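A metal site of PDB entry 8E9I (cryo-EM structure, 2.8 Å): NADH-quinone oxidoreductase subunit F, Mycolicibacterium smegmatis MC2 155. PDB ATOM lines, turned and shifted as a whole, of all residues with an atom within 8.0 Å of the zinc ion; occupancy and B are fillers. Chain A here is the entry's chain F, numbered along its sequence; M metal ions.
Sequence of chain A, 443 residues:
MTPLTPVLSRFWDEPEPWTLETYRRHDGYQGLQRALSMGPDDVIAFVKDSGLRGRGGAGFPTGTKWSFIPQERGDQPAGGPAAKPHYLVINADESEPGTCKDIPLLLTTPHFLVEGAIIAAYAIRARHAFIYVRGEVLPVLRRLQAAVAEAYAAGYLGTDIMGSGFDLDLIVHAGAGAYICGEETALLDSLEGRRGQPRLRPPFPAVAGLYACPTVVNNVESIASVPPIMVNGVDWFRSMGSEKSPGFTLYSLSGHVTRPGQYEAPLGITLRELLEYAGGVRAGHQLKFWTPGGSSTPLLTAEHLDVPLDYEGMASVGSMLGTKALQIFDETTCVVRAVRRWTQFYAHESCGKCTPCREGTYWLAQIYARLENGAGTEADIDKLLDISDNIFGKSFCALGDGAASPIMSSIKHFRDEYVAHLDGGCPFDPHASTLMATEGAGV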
ATOM      1  N   THR A 333     -12.633  -6.164   7.615  1.00  0.00           N
ATOM      2  CA  THR A 333     -12.357  -6.525   6.232  1.00  0.00           C
ATOM      3  C   THR A 333     -11.249  -5.651   5.658  1.00  0.00           C
ATOM      4  O   THR A 333     -11.108  -4.470   6.000  1.00  0.00           O
ATOM      5  CB  THR A 333     -13.599  -6.379   5.372  1.00  0.00           C
ATOM      6  OG1 THR A 333     -13.942  -4.989   5.247  1.00  0.00           O
ATOM      7  CG2 THR A 333     -14.770  -7.126   5.991  1.00  0.00           C
ATOM      8  N   CYS A 334     -10.459  -6.249   4.777  1.00  0.00           N
ATOM      9  CA  CYS A 334      -9.392  -5.554   4.075  1.00  0.00           C
ATOM     10  C   CYS A 334      -9.898  -5.105   2.707  1.00  0.00           C
ATOM     11  O   CYS A 334     -10.345  -5.930   1.904  1.00  0.00           O
ATOM     12  CB  CYS A 334      -8.177  -6.468   3.895  1.00  0.00           C
ATOM     13  SG  CYS A 334      -6.945  -5.845   2.761  1.00  0.00           S
ATOM     14  N   VAL A 335      -9.815  -3.806   2.450  1.00  0.00           N
ATOM     15  CA  VAL A 335     -10.309  -3.284   1.178  1.00  0.00           C
ATOM     16  C   VAL A 335      -9.590  -3.978   0.026  1.00  0.00           C
ATOM     17  O   VAL A 335     -10.206  -4.356  -0.975  1.00  0.00           O
ATOM     18  CB  VAL A 335     -10.131  -1.763   1.111  1.00  0.00           C
ATOM     19  CG1 VAL A 335     -10.513  -1.255  -0.258  1.00  0.00           C
ATOM     20  CG2 VAL A 335     -10.968  -1.086   2.180  1.00  0.00           C
ATOM     21  N   VAL A 336      -8.280  -4.161   0.153  1.00  0.00           N
ATOM     22  CA  VAL A 336      -7.527  -4.790  -0.920  1.00  0.00           C
ATOM     23  C   VAL A 336      -8.009  -6.219  -1.134  1.00  0.00           C
ATOM     24  O   VAL A 336      -8.129  -6.680  -2.277  1.00  0.00           O
ATOM     25  CB  VAL A 336      -6.013  -4.757  -0.620  1.00  0.00           C
ATOM     26  CG1 VAL A 336      -5.233  -5.365  -1.761  1.00  0.00           C
ATOM     27  CG2 VAL A 336      -5.561  -3.336  -0.346  1.00  0.00           C
ATOM     28  N   ARG A 337      -8.291  -6.941  -0.057  1.00  0.00           N
ATOM     29  CA  ARG A 337      -8.772  -8.316  -0.183  1.00  0.00           C
ATOM     30  C   ARG A 337     -10.089  -8.375  -0.945  1.00  0.00           C
ATOM     31  O   ARG A 337     -10.258  -9.185  -1.863  1.00  0.00           O
ATOM     32  CB  ARG A 337      -8.897  -8.920   1.212  1.00  0.00           C
ATOM     33  CG  ARG A 337      -9.491 -10.297   1.307  1.00  0.00           C
ATOM     34  CD  ARG A 337      -9.310 -10.796   2.739  1.00  0.00           C
ATOM     35  NE  ARG A 337     -10.417 -11.614   3.221  1.00  0.00           N
ATOM     36  CZ  ARG A 337     -10.693 -12.836   2.809  1.00  0.00           C
ATOM     37  NH1 ARG A 337      -9.966 -13.427   1.879  1.00  0.00           N
ATOM     38  NH2 ARG A 337     -11.718 -13.487   3.336  1.00  0.00           N
ATOM     39  N   ALA A 338     -11.037  -7.515  -0.577  1.00  0.00           N
ATOM     40  CA  ALA A 338     -12.334  -7.503  -1.236  1.00  0.00           C
ATOM     41  C   ALA A 338     -12.202  -7.108  -2.694  1.00  0.00           C
ATOM     42  O   ALA A 338     -12.805  -7.723  -3.576  1.00  0.00           O
ATOM     43  CB  ALA A 338     -13.278  -6.569  -0.504  1.00  0.00           C
ATOM     44  N   VAL A 339     -11.404  -6.080  -2.974  1.00  0.00           N
ATOM     45  CA  VAL A 339     -11.242  -5.626  -4.346  1.00  0.00           C
ATOM     46  C   VAL A 339     -10.524  -6.687  -5.171  1.00  0.00           C
ATOM     47  O   VAL A 339     -10.802  -6.852  -6.360  1.00  0.00           O
ATOM     48  CB  VAL A 339     -10.512  -4.284  -4.382  1.00  0.00           C
ATOM     49  CG1 VAL A 339     -10.246  -3.860  -5.810  1.00  0.00           C
ATOM     50  CG2 VAL A 339     -11.339  -3.232  -3.673  1.00  0.00           C
ATOM     51  N   ARG A 340      -9.572  -7.402  -4.571  1.00  0.00           N
ATOM     52  CA  ARG A 340      -8.910  -8.492  -5.268  1.00  0.00           C
ATOM     53  C   ARG A 340      -9.891  -9.570  -5.641  1.00  0.00           C
ATOM     54  O   ARG A 340      -9.872 -10.094  -6.757  1.00  0.00           O
ATOM     55  CB  ARG A 340      -7.794  -9.075  -4.410  1.00  0.00           C
ATOM     56  CG  ARG A 340      -7.211 -10.352  -4.999  1.00  0.00           C
ATOM     57  CD  ARG A 340      -6.155 -10.961  -4.135  1.00  0.00           C
ATOM     58  NE  ARG A 340      -5.736 -12.263  -4.655  1.00  0.00           N
ATOM     59  CZ  ARG A 340      -5.144 -13.206  -3.928  1.00  0.00           C
ATOM     60  NH1 ARG A 340      -4.870 -13.022  -2.653  1.00  0.00           N
ATOM     61  NH2 ARG A 340      -4.836 -14.362  -4.506  1.00  0.00           N
ATOM     62  N   TYR A 368      -3.151  -7.583  -7.809  1.00  0.00           N
ATOM     63  CA  TYR A 368      -3.756  -7.708  -6.487  1.00  0.00           C
ATOM     64  C   TYR A 368      -3.291  -8.964  -5.789  1.00  0.00           C
ATOM     65  O   TYR A 368      -3.127  -8.983  -4.566  1.00  0.00           O
ATOM     66  CB  TYR A 368      -5.280  -7.705  -6.616  1.00  0.00           C
ATOM     67  CG  TYR A 368      -5.865  -6.332  -6.534  1.00  0.00           C
ATOM     68  CD1 TYR A 368      -6.040  -5.698  -5.314  1.00  0.00           C
ATOM     69  CD2 TYR A 368      -6.246  -5.652  -7.680  1.00  0.00           C
ATOM     70  CE1 TYR A 368      -6.576  -4.444  -5.236  1.00  0.00           C
ATOM     71  CE2 TYR A 368      -6.783  -4.398  -7.602  1.00  0.00           C
ATOM     72  CZ  TYR A 368      -6.951  -3.797  -6.385  1.00  0.00           C
ATOM     73  OH  TYR A 368      -7.488  -2.544  -6.325  1.00  0.00           O
ATOM     74  N   LEU A 371      -0.196  -7.960  -4.258  1.00  0.00           N
ATOM     75  CA  LEU A 371      -0.435  -7.099  -3.100  1.00  0.00           C
ATOM     76  C   LEU A 371      -0.816  -7.918  -1.876  1.00  0.00           C
ATOM     77  O   LEU A 371      -0.235  -7.744  -0.803  1.00  0.00           O
ATOM     78  CB  LEU A 371      -1.529  -6.079  -3.406  1.00  0.00           C
ATOM     79  CG  LEU A 371      -1.089  -4.820  -4.150  1.00  0.00           C
ATOM     80  CD1 LEU A 371      -2.285  -3.964  -4.470  1.00  0.00           C
ATOM     81  CD2 LEU A 371      -0.097  -4.046  -3.316  1.00  0.00           C
ATOM     82  N   GLU A 372      -1.791  -8.817  -2.015  1.00  0.00           N
ATOM     83  CA  GLU A 372      -2.204  -9.621  -0.883  1.00  0.00           C
ATOM     84  C   GLU A 372      -1.076 -10.505  -0.382  1.00  0.00           C
ATOM     85  O   GLU A 372      -0.915 -10.672   0.831  1.00  0.00           O
ATOM     86  CB  GLU A 372      -3.411 -10.474  -1.245  1.00  0.00           C
ATOM     87  CG  GLU A 372      -4.728  -9.710  -1.237  1.00  0.00           C
ATOM     88  CD  GLU A 372      -5.187  -9.338   0.150  1.00  0.00           C
ATOM     89  OE1 GLU A 372      -5.383 -10.239   0.982  1.00  0.00           O
ATOM     90  OE2 GLU A 372      -5.351  -8.125   0.408  1.00  0.00           O
ATOM     91  N   ASN A 373      -0.299 -11.087  -1.293  1.00  0.00           N
ATOM     92  CA  ASN A 373       0.882 -11.829  -0.912  1.00  0.00           C
ATOM     93  C   ASN A 373       1.979 -10.855  -0.490  1.00  0.00           C
ATOM     94  O   ASN A 373       1.784  -9.639  -0.439  1.00  0.00           O
ATOM     95  CB  ASN A 373       1.332 -12.716  -2.062  1.00  0.00           C
ATOM     96  CG  ASN A 373       0.253 -13.656  -2.534  1.00  0.00           C
ATOM     97  OD1 ASN A 373      -0.707 -13.920  -1.806  1.00  0.00           O
ATOM     98  ND2 ASN A 373       0.401 -14.169  -3.746  1.00  0.00           N
ATOM     99  N   GLU A 417      -4.424   2.219   3.112  1.00  0.00           N
ATOM    100  CA  GLU A 417      -4.439   0.778   3.348  1.00  0.00           C
ATOM    101  C   GLU A 417      -3.705   0.032   2.246  1.00  0.00           C
ATOM    102  O   GLU A 417      -3.002  -0.948   2.506  1.00  0.00           O
ATOM    103  CB  GLU A 417      -5.884   0.300   3.466  1.00  0.00           C
ATOM    104  CG  GLU A 417      -6.056  -1.199   3.478  1.00  0.00           C
ATOM    105  CD  GLU A 417      -7.498  -1.592   3.710  1.00  0.00           C
ATOM    106  OE1 GLU A 417      -8.255  -0.769   4.274  1.00  0.00           O
ATOM    107  OE2 GLU A 417      -7.878  -2.726   3.337  1.00  0.00           O
ATOM    108  N   HIS A 421      -0.460  -2.445   2.724  1.00  0.00           N
ATOM    109  CA  HIS A 421      -0.286  -3.794   2.187  1.00  0.00           C
ATOM    110  C   HIS A 421       1.097  -4.001   1.582  1.00  0.00           C
ATOM    111  O   HIS A 421       1.449  -5.137   1.254  1.00  0.00           O
ATOM    112  CB  HIS A 421      -1.360  -4.089   1.148  1.00  0.00           C
ATOM    113  CG  HIS A 421      -2.628  -4.617   1.730  1.00  0.00           C
ATOM    114  ND1 HIS A 421      -3.449  -3.848   2.516  1.00  0.00           N
ATOM    115  CD2 HIS A 421      -3.221  -5.835   1.643  1.00  0.00           C
ATOM    116  CE1 HIS A 421      -4.493  -4.561   2.905  1.00  0.00           C
ATOM    117  NE2 HIS A 421      -4.371  -5.773   2.382  1.00  0.00           N
ATOM    118  N   GLY A 425       2.381  -7.715   2.952  1.00  0.00           N
ATOM    119  CA  GLY A 425       1.134  -8.416   2.718  1.00  0.00           C
ATOM    120  C   GLY A 425      -0.037  -7.763   3.436  1.00  0.00           C
ATOM    121  O   GLY A 425       0.056  -6.660   3.967  1.00  0.00           O
ATOM    122  N   CYS A 426      -1.152  -8.478   3.457  1.00  0.00           N
ATOM    123  CA  CYS A 426      -2.334  -7.982   4.136  1.00  0.00           C
ATOM    124  C   CYS A 426      -2.153  -8.111   5.641  1.00  0.00           C
ATOM    125  O   CYS A 426      -1.989  -9.229   6.141  1.00  0.00           O
ATOM    126  CB  CYS A 426      -3.575  -8.744   3.693  1.00  0.00           C
ATOM    127  SG  CYS A 426      -5.118  -8.008   4.279  1.00  0.00           S
ATOM    128  N   PRO A 427      -2.192  -7.017   6.401  1.00  0.00           N
ATOM    129  CA  PRO A 427      -2.116  -7.148   7.859  1.00  0.00           C
ATOM    130  C   PRO A 427      -3.329  -7.848   8.448  1.00  0.00           C
ATOM    131  O   PRO A 427      -3.198  -8.564   9.443  1.00  0.00           O
ATOM    132  CB  PRO A 427      -2.010  -5.704   8.343  1.00  0.00           C
ATOM    133  CG  PRO A 427      -2.682  -4.906   7.284  1.00  0.00           C
ATOM    134  CD  PRO A 427      -2.386  -5.613   5.988  1.00  0.00           C
ATOM    135  N   PHE A 428      -4.499  -7.676   7.837  1.00  0.00           N
ATOM    136  CA  PHE A 428      -5.738  -8.167   8.426  1.00  0.00           C
ATOM    137  C   PHE A 428      -5.723  -9.680   8.557  1.00  0.00           C
ATOM    138  O   PHE A 428      -5.060 -10.384   7.791  1.00  0.00           O
ATOM    139  CB  PHE A 428      -6.921  -7.734   7.579  1.00  0.00           C
ATOM    140  CG  PHE A 428      -7.128  -6.242   7.542  1.00  0.00           C
ATOM    141  CD1 PHE A 428      -8.035  -5.648   8.395  1.00  0.00           C
ATOM    142  CD2 PHE A 428      -6.385  -5.449   6.699  1.00  0.00           C
ATOM    143  CE1 PHE A 428      -8.218  -4.289   8.368  1.00  0.00           C
ATOM    144  CE2 PHE A 428      -6.568  -4.089   6.673  1.00  0.00           C
ATOM    145  CZ  PHE A 428      -7.482  -3.502   7.515  1.00  0.00           C
ATOM    146  N   ASP A 429      -6.443 -10.175   9.558  1.00  0.00           N
ATOM    147  CA  ASP A 429      -6.642 -11.597   9.728  1.00  0.00           C
ATOM    148  C   ASP A 429      -7.981 -11.990   9.118  1.00  0.00           C
ATOM    149  O   ASP A 429      -9.026 -11.499   9.576  1.00  0.00           O
ATOM    150  CB  ASP A 429      -6.603 -11.976  11.192  1.00  0.00           C
ATOM    151  N   PRO A 430      -8.019 -12.855   8.116  1.00  0.00           N
ATOM    152  CA  PRO A 430      -9.310 -13.203   7.505  1.00  0.00           C
ATOM    153  C   PRO A 430     -10.324 -13.752   8.487  1.00  0.00           C
ATOM    154  O   PRO A 430     -11.521 -13.502   8.324  1.00  0.00           O
ATOM    155  CB  PRO A 430      -8.925 -14.254   6.449  1.00  0.00           C
ATOM    156  CG  PRO A 430      -7.513 -13.951   6.122  1.00  0.00           C
ATOM    157  CD  PRO A 430      -6.895 -13.493   7.399  1.00  0.00           C
HETATM  158 ZN    ZN M   1      -5.684  -7.634   2.084  1.00  0.00          ZN
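The zinc ion is bound by OE2 of Glu 372 (1.8 Å). The zinc ion is bound by SG of Cys 334, 2.3 Å away. A ring nitrogen (NE2) of His 421 is bound to the zinc ion (2.3 Å). The side-chain sulfur (SG) of Cys 426 is bound to the zinc ion, 2.3 Å away. Slightly farther from the zinc ion lies the side-chain carboxylate (OE1) of Glu 372 (2.8 Å).
Val 336 touches the zinc ion (CB to ZN, 3.96 Å). Arg 337 touches the zinc ion (N to ZN, 3.4 Å).
The side-chain carboxylate of Glu 372 sits close to the backbone NH of Arg 337 (3.2 Å). The side-chain sulfur of Cys 334 sits close to the backbone NH of Arg 337, at 3.3 Å. The backbone NH (N) of Val 336 sits close to the side-chain sulfur (SG) of Cys 334 (3.4 Å). The side-chain sulfur (SG) of Cys 334 sits close to the side-chain carboxylate (OE2) of Glu 417 (3.3 Å). A ring nitrogen (ND1) of His 421 is in hydrogen-bond range of the backbone carbonyl oxygen (O) of Glu 417, 2.9 Å away. N of Phe 428 lies close to SG of Cys 426 (3.6 Å).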
